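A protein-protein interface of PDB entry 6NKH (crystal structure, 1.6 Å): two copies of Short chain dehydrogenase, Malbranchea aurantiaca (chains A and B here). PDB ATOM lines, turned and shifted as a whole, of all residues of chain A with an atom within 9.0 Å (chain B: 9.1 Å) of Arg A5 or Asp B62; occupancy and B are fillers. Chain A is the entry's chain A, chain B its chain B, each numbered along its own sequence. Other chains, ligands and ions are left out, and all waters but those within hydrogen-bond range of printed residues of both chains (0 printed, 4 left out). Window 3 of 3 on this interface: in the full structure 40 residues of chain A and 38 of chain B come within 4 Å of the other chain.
Thr A4 touches its own counterpart, Thr B4. Thr A4 touches His B36, and with the chains exchanged His A36 touches Thr B4. 3 positions are printed for both chains. Of the 7 pairs that touch across the chains among the printed residues, 3 have their exchanged pair printed and touching as well.
Hydrophobic or aromatic side chains of chain B within 4 Å of the printed part of chain A: His B36. Of the 11 printed residues of chain A, 5 touch a printed residue of chain B. Among the printed residues, 7 pairs touch across the chains.
Among the printed residues, merely in contact across the chains: Thr A4 with Glu B35 (3.8 Å), Thr A4 with His B36 (3.6 Å), Leu A10 with Glu B239 (3.98 Å), His A36 with Thr B4 (3.6 Å) and Lys A246 with Glu B239 (3.4 Å).
OD2 of Asp A9 is in salt-bridge range of NH1 of Arg A5, 2.9 Å away. The side-chain amino group of Lys A246 lies within hydrogen-bond range of the side-chain hydroxyl of Ser A7. NE2 of His A36 lies within hydrogen-bond range of NZ of Lys A246 (3.4 Å). The backbone carbonyl oxygen (O) of Leu B32 lies within hydrogen-bond range of a ring nitrogen (ND1) of His B36 (2.5 Å). OE2 of Glu B35 sits at hydrogen-bond distance from NE2 of His B60.
Of chain B, only Asp B62 comes within 4 Å of Arg A5. Of chain A, only Arg A5 comes within 4 Å of Asp B62. Of chain B, only Thr B4 (2.6 Å), Glu B35 (3.8 Å) and His B36 (3.6 Å) come within 4 Å of Thr A4. Printed residues of chain A within 4 Å of Glu B35: Thr A4 (3.8 Å). Pro B61 touches none of the printed residues of chain A. Printed residues of chain B within 4 Å of Leu A10: Glu B239. Printed residues of chain A within 4 Å of Glu B239: Leu A10 (3.98 Å) and Lys A246 (3.4 Å). Printed residues of chain A within 4 Å of His B36: Thr A4. Of the printed residues of chain B, His A36 touches Thr B4. Of the printed residues of chain B, Lys A246 touches Glu B239. Gln B31 touches none of the printed residues of chain A. The nearest residue of chain B that does not touch Arg A5 is Arg B8 (5.2 Å).
N of Thr B4 sits close to N of Thr A4, 2.6 Å away. The guanidinium group (NH2) of Arg A5 lies within salt-bridge range of the side-chain carboxylate (OD1) of Asp B62 (2.8 Å).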
ATOM      1  N   THR A   4      -2.688  12.115  17.204  1.00  0.00           N
ATOM      2  CA  THR A   4      -2.186  11.392  16.048  1.00  0.00           C
ATOM      3  C   THR A   4      -1.395  12.382  15.203  1.00  0.00           C
ATOM      4  O   THR A   4      -1.483  13.586  15.426  1.00  0.00           O
ATOM      5  CB  THR A   4      -3.321  10.765  15.234  1.00  0.00           C
ATOM      6  OG1 THR A   4      -4.049  11.778  14.524  1.00  0.00           O
ATOM      7  CG2 THR A   4      -4.266  10.031  16.170  1.00  0.00           C
ATOM      8  N   ARG A   5      -0.637  11.887  14.220  1.00  0.00           N
ATOM      9  CA  ARG A   5       0.289  12.771  13.523  1.00  0.00           C
ATOM     10  C   ARG A   5      -0.447  13.789  12.653  1.00  0.00           C
ATOM     11  O   ARG A   5       0.009  14.931  12.532  1.00  0.00           O
ATOM     12  CB  ARG A   5       1.296  11.979  12.683  1.00  0.00           C
ATOM     13  CG  ARG A   5       2.304  12.909  12.022  1.00  0.00           C
ATOM     14  CD  ARG A   5       3.292  12.202  11.148  1.00  0.00           C
ATOM     15  NE  ARG A   5       2.642  11.250  10.258  1.00  0.00           N
ATOM     16  CZ  ARG A   5       1.812  11.568   9.271  1.00  0.00           C
ATOM     17  NH1 ARG A   5       1.466  12.831   9.051  1.00  0.00           N
ATOM     18  NH2 ARG A   5       1.295  10.607   8.520  1.00  0.00           N
ATOM     19  N   ARG A   6      -1.582  13.422  12.039  1.00  0.00           N
ATOM     20  CA  ARG A   6      -2.229  14.391  11.153  1.00  0.00           C
ATOM     21  C   ARG A   6      -2.899  15.514  11.940  1.00  0.00           C
ATOM     22  O   ARG A   6      -2.792  16.683  11.555  1.00  0.00           O
ATOM     23  CB  ARG A   6      -3.227  13.736  10.198  1.00  0.00           C
ATOM     24  CG  ARG A   6      -3.878  14.783   9.275  1.00  0.00           C
ATOM     25  CD  ARG A   6      -2.841  15.758   8.663  1.00  0.00           C
ATOM     26  NE  ARG A   6      -1.767  15.101   7.921  1.00  0.00           N
ATOM     27  CZ  ARG A   6      -1.788  14.862   6.614  1.00  0.00           C
ATOM     28  NH1 ARG A   6      -2.825  15.240   5.878  1.00  0.00           N
ATOM     29  NH2 ARG A   6      -0.757  14.255   6.044  1.00  0.00           N
ATOM     30  N   SER A   7      -3.570  15.204  13.052  1.00  0.00           N
ATOM     31  CA  SER A   7      -4.006  16.279  13.943  1.00  0.00           C
ATOM     32  C   SER A   7      -2.813  17.115  14.387  1.00  0.00           C
ATOM     33  O   SER A   7      -2.890  18.348  14.454  1.00  0.00           O
ATOM     34  CB  SER A   7      -4.732  15.701  15.156  1.00  0.00           C
ATOM     35  OG  SER A   7      -5.943  15.080  14.772  1.00  0.00           O
ATOM     36  N   ARG A   8      -1.687  16.442  14.664  1.00  0.00           N
ATOM     37  CA  ARG A   8      -0.472  17.103  15.132  1.00  0.00           C
ATOM     38  C   ARG A   8       0.075  18.025  14.053  1.00  0.00           C
ATOM     39  O   ARG A   8       0.516  19.143  14.340  1.00  0.00           O
ATOM     40  CB  ARG A   8       0.562  16.035  15.506  1.00  0.00           C
ATOM     41  CG  ARG A   8       1.533  16.387  16.621  1.00  0.00           C
ATOM     42  CD  ARG A   8       2.412  15.175  16.913  1.00  0.00           C
ATOM     43  NE  ARG A   8       3.256  14.850  15.766  1.00  0.00           N
ATOM     44  CZ  ARG A   8       4.039  13.778  15.685  1.00  0.00           C
ATOM     45  NH1 ARG A   8       4.093  12.916  16.689  1.00  0.00           N
ATOM     46  NH2 ARG A   8       4.770  13.570  14.598  1.00  0.00           N
ATOM     47  N   ASP A   9       0.013  17.581  12.793  1.00  0.00           N
ATOM     48  CA  ASP A   9       0.501  18.369  11.670  1.00  0.00           C
ATOM     49  C   ASP A   9      -0.475  19.474  11.299  1.00  0.00           C
ATOM     50  O   ASP A   9      -0.050  20.535  10.832  1.00  0.00           O
ATOM     51  CB  ASP A   9       0.780  17.457  10.468  1.00  0.00           C
ATOM     52  CG  ASP A   9       1.948  16.521  10.720  1.00  0.00           C
ATOM     53  OD1 ASP A   9       2.818  16.857  11.556  1.00  0.00           O
ATOM     54  OD2 ASP A   9       1.999  15.448  10.083  1.00  0.00           O
ATOM     55  N   LEU A  10      -1.776  19.259  11.508  1.00  0.00           N
ATOM     56  CA  LEU A  10      -2.733  20.349  11.344  1.00  0.00           C
ATOM     57  C   LEU A  10      -2.375  21.530  12.243  1.00  0.00           C
ATOM     58  O   LEU A  10      -2.487  22.688  11.824  1.00  0.00           O
ATOM     59  CB  LEU A  10      -4.159  19.859  11.625  1.00  0.00           C
ATOM     60  CG  LEU A  10      -4.863  18.985  10.578  1.00  0.00           C
ATOM     61  CD1 LEU A  10      -6.115  18.305  11.130  1.00  0.00           C
ATOM     62  CD2 LEU A  10      -5.253  19.817   9.367  1.00  0.00           C
ATOM     63  N   LEU A  11      -1.872  21.265  13.457  1.00  0.00           N
ATOM     64  CA  LEU A  11      -1.694  22.327  14.437  1.00  0.00           C
ATOM     65  C   LEU A  11      -0.292  22.497  15.021  1.00  0.00           C
ATOM     66  O   LEU A  11      -0.100  23.457  15.771  1.00  0.00           O
ATOM     67  CB  LEU A  11      -2.682  22.131  15.601  1.00  0.00           C
ATOM     68  CG  LEU A  11      -4.145  22.426  15.279  1.00  0.00           C
ATOM     69  CD1 LEU A  11      -5.093  21.927  16.352  1.00  0.00           C
ATOM     70  CD2 LEU A  11      -4.337  23.921  15.088  1.00  0.00           C
ATOM     71  N   ARG A  12       0.691  21.632  14.720  1.00  0.00           N
ATOM     72  CA  ARG A  12       2.037  21.867  15.254  1.00  0.00           C
ATOM     73  C   ARG A  12       2.597  23.180  14.721  1.00  0.00           C
ATOM     74  O   ARG A  12       2.459  23.491  13.535  1.00  0.00           O
ATOM     75  CB  ARG A  12       3.052  20.749  14.935  1.00  0.00           C
ATOM     76  CG  ARG A  12       3.013  19.571  15.905  1.00  0.00           C
ATOM     77  CD  ARG A  12       4.117  18.490  15.745  1.00  0.00           C
ATOM     78  NE  ARG A  12       5.000  18.335  16.909  1.00  0.00           N
ATOM     79  CZ  ARG A  12       6.004  17.459  16.974  1.00  0.00           C
ATOM     80  NH1 ARG A  12       6.271  16.671  15.942  1.00  0.00           N
ATOM     81  NH2 ARG A  12       6.736  17.348  18.075  1.00  0.00           N
ATOM     82  N   HIS A  36      -1.453  19.183  21.059  1.00  0.00           N
ATOM     83  CA  HIS A  36      -1.317  18.983  19.620  1.00  0.00           C
ATOM     84  C   HIS A  36      -0.088  19.670  19.035  1.00  0.00           C
ATOM     85  O   HIS A  36       0.060  19.708  17.810  1.00  0.00           O
ATOM     86  CB  HIS A  36      -2.578  19.480  18.895  1.00  0.00           C
ATOM     87  CG  HIS A  36      -3.762  18.569  19.031  1.00  0.00           C
ATOM     88  ND1 HIS A  36      -4.586  18.574  20.134  1.00  0.00           N
ATOM     89  CD2 HIS A  36      -4.279  17.651  18.180  1.00  0.00           C
ATOM     90  CE1 HIS A  36      -5.547  17.681  19.968  1.00  0.00           C
ATOM     91  NE2 HIS A  36      -5.384  17.109  18.788  1.00  0.00           N
ATOM     92  N   LYS A 246      -9.367  22.272  12.918  1.00  0.00           N
ATOM     93  CA  LYS A 246      -8.920  21.189  12.049  1.00  0.00           C
ATOM     94  C   LYS A 246      -9.689  21.140  10.729  1.00  0.00           C
ATOM     95  O   LYS A 246      -9.107  20.824   9.683  1.00  0.00           O
ATOM     96  CB  LYS A 246      -9.073  19.851  12.782  1.00  0.00           C
ATOM     97  CG  LYS A 246      -8.163  19.661  13.983  1.00  0.00           C
ATOM     98  CD  LYS A 246      -8.434  18.318  14.634  1.00  0.00           C
ATOM     99  CE  LYS A 246      -7.577  18.101  15.862  1.00  0.00           C
ATOM    100  NZ  LYS A 246      -7.878  16.783  16.499  1.00  0.00           N
ATOM    101  N   THR B   4      -3.030  12.518  19.735  1.00  0.00           N
ATOM    102  CA  THR B   4      -2.635  12.776  21.108  1.00  0.00           C
ATOM    103  C   THR B   4      -3.135  11.639  21.999  1.00  0.00           C
ATOM    104  O   THR B   4      -4.036  10.891  21.618  1.00  0.00           O
ATOM    105  CB  THR B   4      -3.189  14.111  21.602  1.00  0.00           C
ATOM    106  OG1 THR B   4      -4.611  14.032  21.729  1.00  0.00           O
ATOM    107  CG2 THR B   4      -2.862  15.206  20.608  1.00  0.00           C
ATOM    108  N   ARG B   8      -6.541   9.152  21.590  1.00  0.00           N
ATOM    109  CA  ARG B   8      -6.370   7.702  21.526  1.00  0.00           C
ATOM    110  C   ARG B   8      -7.118   7.031  22.665  1.00  0.00           C
ATOM    111  O   ARG B   8      -7.763   5.993  22.474  1.00  0.00           O
ATOM    112  CB  ARG B   8      -4.885   7.323  21.585  1.00  0.00           C
ATOM    113  CG  ARG B   8      -4.089   7.798  20.396  1.00  0.00           C
ATOM    114  CD  ARG B   8      -2.637   7.345  20.417  1.00  0.00           C
ATOM    115  NE  ARG B   8      -1.953   7.855  19.227  1.00  0.00           N
ATOM    116  CZ  ARG B   8      -0.702   7.571  18.870  1.00  0.00           C
ATOM    117  NH1 ARG B   8       0.046   6.752  19.601  1.00  0.00           N
ATOM    118  NH2 ARG B   8      -0.200   8.104  17.760  1.00  0.00           N
ATOM    119  N   ALA B  30     -13.262   6.195   8.276  1.00  0.00           N
ATOM    120  CA  ALA B  30     -12.609   4.944   8.646  1.00  0.00           C
ATOM    121  C   ALA B  30     -11.116   5.152   8.849  1.00  0.00           C
ATOM    122  O   ALA B  30     -10.529   4.602   9.783  1.00  0.00           O
ATOM    123  CB  ALA B  30     -12.876   3.877   7.582  1.00  0.00           C
ATOM    124  N   GLN B  31     -10.486   5.965   8.000  1.00  0.00           N
ATOM    125  CA  GLN B  31      -9.064   6.247   8.166  1.00  0.00           C
ATOM    126  C   GLN B  31      -8.777   6.896   9.510  1.00  0.00           C
ATOM    127  O   GLN B  31      -7.865   6.479  10.227  1.00  0.00           O
ATOM    128  CB  GLN B  31      -8.560   7.143   7.035  1.00  0.00           C
ATOM    129  CG  GLN B  31      -8.376   6.435   5.714  1.00  0.00           C
ATOM    130  CD  GLN B  31      -7.898   7.369   4.619  1.00  0.00           C
ATOM    131  OE1 GLN B  31      -7.876   8.587   4.792  1.00  0.00           O
ATOM    132  NE2 GLN B  31      -7.479   6.800   3.497  1.00  0.00           N
ATOM    133  N   LEU B  32      -9.524   7.944   9.860  1.00  0.00           N
ATOM    134  CA  LEU B  32      -9.234   8.658  11.099  1.00  0.00           C
ATOM    135  C   LEU B  32      -9.428   7.769  12.322  1.00  0.00           C
ATOM    136  O   LEU B  32      -8.669   7.870  13.289  1.00  0.00           O
ATOM    137  CB  LEU B  32     -10.098   9.913  11.212  1.00  0.00           C
ATOM    138  CG  LEU B  32      -9.697  11.123  10.372  1.00  0.00           C
ATOM    139  CD1 LEU B  32     -10.732  12.221  10.492  1.00  0.00           C
ATOM    140  CD2 LEU B  32      -8.353  11.644  10.821  1.00  0.00           C
ATOM    141  N   VAL B  33     -10.433   6.889  12.304  1.00  0.00           N
ATOM    142  CA  VAL B  33     -10.705   6.093  13.497  1.00  0.00           C
ATOM    143  C   VAL B  33      -9.657   5.001  13.676  1.00  0.00           C
ATOM    144  O   VAL B  33      -9.349   4.617  14.809  1.00  0.00           O
ATOM    145  CB  VAL B  33     -12.133   5.502  13.476  1.00  0.00           C
ATOM    146  CG1 VAL B  33     -13.174   6.617  13.407  1.00  0.00           C
ATOM    147  CG2 VAL B  33     -12.335   4.514  12.344  1.00  0.00           C
ATOM    148  N   ILE B  34      -9.075   4.491  12.589  1.00  0.00           N
ATOM    149  CA  ILE B  34      -8.033   3.478  12.754  1.00  0.00           C
ATOM    150  C   ILE B  34      -6.715   4.123  13.160  1.00  0.00           C
ATOM    151  O   ILE B  34      -5.907   3.503  13.859  1.00  0.00           O
ATOM    152  CB  ILE B  34      -7.875   2.627  11.482  1.00  0.00           C
ATOM    153  CG1 ILE B  34      -7.476   3.498  10.289  1.00  0.00           C
ATOM    154  CG2 ILE B  34      -9.155   1.851  11.209  1.00  0.00           C
ATOM    155  CD1 ILE B  34      -7.139   2.702   9.037  1.00  0.00           C
ATOM    156  N   GLU B  35      -6.478   5.368  12.748  1.00  0.00           N
ATOM    157  CA  GLU B  35      -5.324   6.106  13.247  1.00  0.00           C
ATOM    158  C   GLU B  35      -5.362   6.222  14.765  1.00  0.00           C
ATOM    159  O   GLU B  35      -4.315   6.360  15.405  1.00  0.00           O
ATOM    160  CB  GLU B  35      -5.280   7.498  12.609  1.00  0.00           C
ATOM    161  CG  GLU B  35      -5.056   7.486  11.096  1.00  0.00           C
ATOM    162  CD  GLU B  35      -5.077   8.879  10.457  1.00  0.00           C
ATOM    163  OE1 GLU B  35      -5.323   9.875  11.174  1.00  0.00           O
ATOM    164  OE2 GLU B  35      -4.865   8.974   9.228  1.00  0.00           O
ATOM    165  N   HIS B  36      -6.559   6.166  15.350  1.00  0.00           N
ATOM    166  CA  HIS B  36      -6.776   6.309  16.784  1.00  0.00           C
ATOM    167  C   HIS B  36      -6.832   4.978  17.523  1.00  0.00           C
ATOM    168  O   HIS B  36      -7.035   4.968  18.740  1.00  0.00           O
ATOM    169  CB  HIS B  36      -8.079   7.091  17.037  1.00  0.00           C
ATOM    170  CG  HIS B  36      -7.980   8.556  16.727  1.00  0.00           C
ATOM    171  ND1 HIS B  36      -8.124   9.063  15.452  1.00  0.00           N
ATOM    172  CD2 HIS B  36      -7.774   9.624  17.535  1.00  0.00           C
ATOM    173  CE1 HIS B  36      -7.986  10.378  15.484  1.00  0.00           C
ATOM    174  NE2 HIS B  36      -7.775  10.744  16.736  1.00  0.00           N
ATOM    175  N   GLY B  37      -6.655   3.861  16.827  1.00  0.00           N
ATOM    176  CA  GLY B  37      -6.705   2.565  17.463  1.00  0.00           C
ATOM    177  C   GLY B  37      -8.078   1.950  17.565  1.00  0.00           C
ATOM    178  O   GLY B  37      -8.257   0.996  18.330  1.00  0.00           O
ATOM    179  N   ALA B  56      -7.346  -1.205   1.034  1.00  0.00           N
ATOM    180  CA  ALA B  56      -6.814   0.145   1.168  1.00  0.00           C
ATOM    181  C   ALA B  56      -6.643   0.515   2.637  1.00  0.00           C
ATOM    182  O   ALA B  56      -5.583   0.997   3.053  1.00  0.00           O
ATOM    183  CB  ALA B  56      -7.737   1.138   0.462  1.00  0.00           C
ATOM    184  N   LEU B  57      -7.679   0.280   3.444  1.00  0.00           N
ATOM    185  CA  LEU B  57      -7.593   0.609   4.862  1.00  0.00           C
ATOM    186  C   LEU B  57      -6.524  -0.219   5.563  1.00  0.00           C
ATOM    187  O   LEU B  57      -5.674   0.326   6.277  1.00  0.00           O
ATOM    188  CB  LEU B  57      -8.951   0.407   5.538  1.00  0.00           C
ATOM    189  CG  LEU B  57     -10.030   1.435   5.211  1.00  0.00           C
ATOM    190  CD1 LEU B  57     -11.349   1.003   5.814  1.00  0.00           C
ATOM    191  CD2 LEU B  57      -9.626   2.821   5.718  1.00  0.00           C
ATOM    192  N   LYS B  58      -6.553  -1.545   5.378  1.00  0.00           N
ATOM    193  CA  LYS B  58      -5.635  -2.408   6.115  1.00  0.00           C
ATOM    194  C   LYS B  58      -4.175  -2.048   5.869  1.00  0.00           C
ATOM    195  O   LYS B  58      -3.318  -2.402   6.685  1.00  0.00           O
ATOM    196  CB  LYS B  58      -5.874  -3.873   5.756  1.00  0.00           C
ATOM    197  CG  LYS B  58      -4.966  -4.844   6.504  1.00  0.00           C
ATOM    198  CD  LYS B  58      -5.359  -6.288   6.231  1.00  0.00           C
ATOM    199  CE  LYS B  58      -4.455  -7.295   6.950  1.00  0.00           C
ATOM    200  NZ  LYS B  58      -3.093  -7.389   6.340  1.00  0.00           N
ATOM    201  N   GLN B  59      -3.873  -1.346   4.781  1.00  0.00           N
ATOM    202  CA  GLN B  59      -2.507  -0.955   4.475  1.00  0.00           C
ATOM    203  C   GLN B  59      -2.206   0.493   4.859  1.00  0.00           C
ATOM    204  O   GLN B  59      -1.088   0.963   4.627  1.00  0.00           O
ATOM    205  CB  GLN B  59      -2.230  -1.158   2.977  1.00  0.00           C
ATOM    206  CG  GLN B  59      -2.584  -2.556   2.428  1.00  0.00           C
ATOM    207  CD  GLN B  59      -1.831  -3.707   3.091  1.00  0.00           C
ATOM    208  OE1 GLN B  59      -0.660  -3.583   3.453  1.00  0.00           O
ATOM    209  NE2 GLN B  59      -2.508  -4.848   3.230  1.00  0.00           N
ATOM    210  N   HIS B  60      -3.164   1.199   5.453  1.00  0.00           N
ATOM    211  CA  HIS B  60      -3.013   2.629   5.704  1.00  0.00           C
ATOM    212  C   HIS B  60      -1.740   2.904   6.500  1.00  0.00           C
ATOM    213  O   HIS B  60      -1.469   2.214   7.495  1.00  0.00           O
ATOM    214  CB  HIS B  60      -4.243   3.142   6.457  1.00  0.00           C
ATOM    215  CG  HIS B  60      -4.262   4.627   6.674  1.00  0.00           C
ATOM    216  ND1 HIS B  60      -4.545   5.526   5.667  1.00  0.00           N
ATOM    217  CD2 HIS B  60      -4.064   5.366   7.791  1.00  0.00           C
ATOM    218  CE1 HIS B  60      -4.508   6.755   6.152  1.00  0.00           C
ATOM    219  NE2 HIS B  60      -4.216   6.685   7.438  1.00  0.00           N
ATOM    220  N   PRO B  61      -0.928   3.899   6.108  1.00  0.00           N
ATOM    221  CA  PRO B  61       0.345   4.119   6.803  1.00  0.00           C
ATOM    222  C   PRO B  61       0.207   4.490   8.278  1.00  0.00           C
ATOM    223  O   PRO B  61       0.803   3.832   9.133  1.00  0.00           O
ATOM    224  CB  PRO B  61       0.990   5.256   5.997  1.00  0.00           C
ATOM    225  CG  PRO B  61       0.367   5.166   4.654  1.00  0.00           C
ATOM    226  CD  PRO B  61      -1.043   4.736   4.897  1.00  0.00           C
ATOM    227  N   ASP B  62      -0.549   5.551   8.587  1.00  0.00           N
ATOM    228  CA  ASP B  62      -0.735   5.999   9.970  1.00  0.00           C
ATOM    229  C   ASP B  62      -1.660   5.088  10.775  1.00  0.00           C
ATOM    230  O   ASP B  62      -1.914   5.382  11.949  1.00  0.00           O
ATOM    231  CB  ASP B  62      -1.278   7.436  10.010  1.00  0.00           C
ATOM    232  CG  ASP B  62      -0.220   8.473   9.681  1.00  0.00           C
ATOM    233  OD1 ASP B  62       0.968   8.216   9.949  1.00  0.00           O
ATOM    234  OD2 ASP B  62      -0.570   9.557   9.164  1.00  0.00           O
ATOM    235  N   ARG B  63      -2.149   3.996  10.183  1.00  0.00           N
ATOM    236  CA  ARG B  63      -2.969   3.040  10.909  1.00  0.00           C
ATOM    237  C   ARG B  63      -2.253   2.544  12.154  1.00  0.00           C
ATOM    238  O   ARG B  63      -1.067   2.206  12.117  1.00  0.00           O
ATOM    239  CB  ARG B  63      -3.314   1.844  10.026  1.00  0.00           C
ATOM    240  CG  ARG B  63      -4.107   0.784  10.764  1.00  0.00           C
ATOM    241  CD  ARG B  63      -4.450  -0.388   9.882  1.00  0.00           C
ATOM    242  NE  ARG B  63      -3.276  -1.190   9.576  1.00  0.00           N
ATOM    243  CZ  ARG B  63      -2.765  -2.105  10.396  1.00  0.00           C
ATOM    244  NH1 ARG B  63      -1.691  -2.784  10.029  1.00  0.00           N
ATOM    245  NH2 ARG B  63      -3.321  -2.341  11.581  1.00  0.00           N
ATOM    246  N   ASP B  64      -2.989   2.478  13.251  1.00  0.00           N
ATOM    247  CA  ASP B  64      -2.434   1.930  14.469  1.00  0.00           C
ATOM    248  C   ASP B  64      -2.292   0.422  14.311  1.00  0.00           C
ATOM    249  O   ASP B  64      -3.188  -0.230  13.770  1.00  0.00           O
ATOM    250  CB  ASP B  64      -3.330   2.232  15.657  1.00  0.00           C
ATOM    251  CG  ASP B  64      -2.628   2.017  16.953  1.00  0.00           C
ATOM    252  OD1 ASP B  64      -1.887   2.934  17.367  1.00  0.00           O
ATOM    253  OD2 ASP B  64      -2.765   0.919  17.522  1.00  0.00           O
ATOM    254  N   PRO B  65      -1.186  -0.161  14.762  1.00  0.00           N
ATOM    255  CA  PRO B  65      -1.031  -1.615  14.599  1.00  0.00           C
ATOM    256  C   PRO B  65      -2.168  -2.426  15.192  1.00  0.00           C
ATOM    257  O   PRO B  65      -2.560  -3.439  14.598  1.00  0.00           O
ATOM    258  CB  PRO B  65       0.304  -1.896  15.301  1.00  0.00           C
ATOM    259  CG  PRO B  65       1.052  -0.613  15.191  1.00  0.00           C
ATOM    260  CD  PRO B  65       0.022   0.467  15.322  1.00  0.00           C
ATOM    261  N   ILE B  66      -2.722  -2.014  16.340  1.00  0.00           N
ATOM    262  CA  ILE B  66      -3.766  -2.813  16.979  1.00  0.00           C
ATOM    263  C   ILE B  66      -5.096  -2.700  16.248  1.00  0.00           C
ATOM    264  O   ILE B  66      -5.969  -3.554  16.428  1.00  0.00           O
ATOM    265  CB  ILE B  66      -3.973  -2.418  18.455  1.00  0.00           C
ATOM    266  CG1 ILE B  66      -4.601  -1.028  18.592  1.00  0.00           C
ATOM    267  CG2 ILE B  66      -2.661  -2.440  19.200  1.00  0.00           C
ATOM    268  CD1 ILE B  66      -6.115  -1.048  18.755  1.00  0.00           C
ATOM    269  N   ALA B  67      -5.271  -1.670  15.425  1.00  0.00           N
ATOM    270  CA  ALA B  67      -6.534  -1.461  14.736  1.00  0.00           C
ATOM    271  C   ALA B  67      -6.787  -2.590  13.748  1.00  0.00           C
ATOM    272  O   ALA B  67      -5.897  -2.975  12.986  1.00  0.00           O
ATOM    273  CB  ALA B  67      -6.530  -0.115  14.017  1.00  0.00           C
ATOM    274  N   GLU B 239     -13.306  15.022   9.902  1.00  0.00           N
ATOM    275  CA  GLU B 239     -12.995  15.495  11.243  1.00  0.00           C
ATOM    276  C   GLU B 239     -14.252  15.808  12.052  1.00  0.00           C
ATOM    277  O   GLU B 239     -14.195  15.818  13.287  1.00  0.00           O
ATOM    278  CB  GLU B 239     -12.108  16.741  11.171  1.00  0.00           C
ATOM    279  CG  GLU B 239     -10.670  16.543  10.620  1.00  0.00           C
ATOM    280  CD  GLU B 239      -9.701  15.828  11.563  1.00  0.00           C
ATOM    281  OE1 GLU B 239      -9.900  15.870  12.798  1.00  0.00           O
ATOM    282  OE2 GLU B 239      -8.696  15.272  11.065  1.00  0.00           O
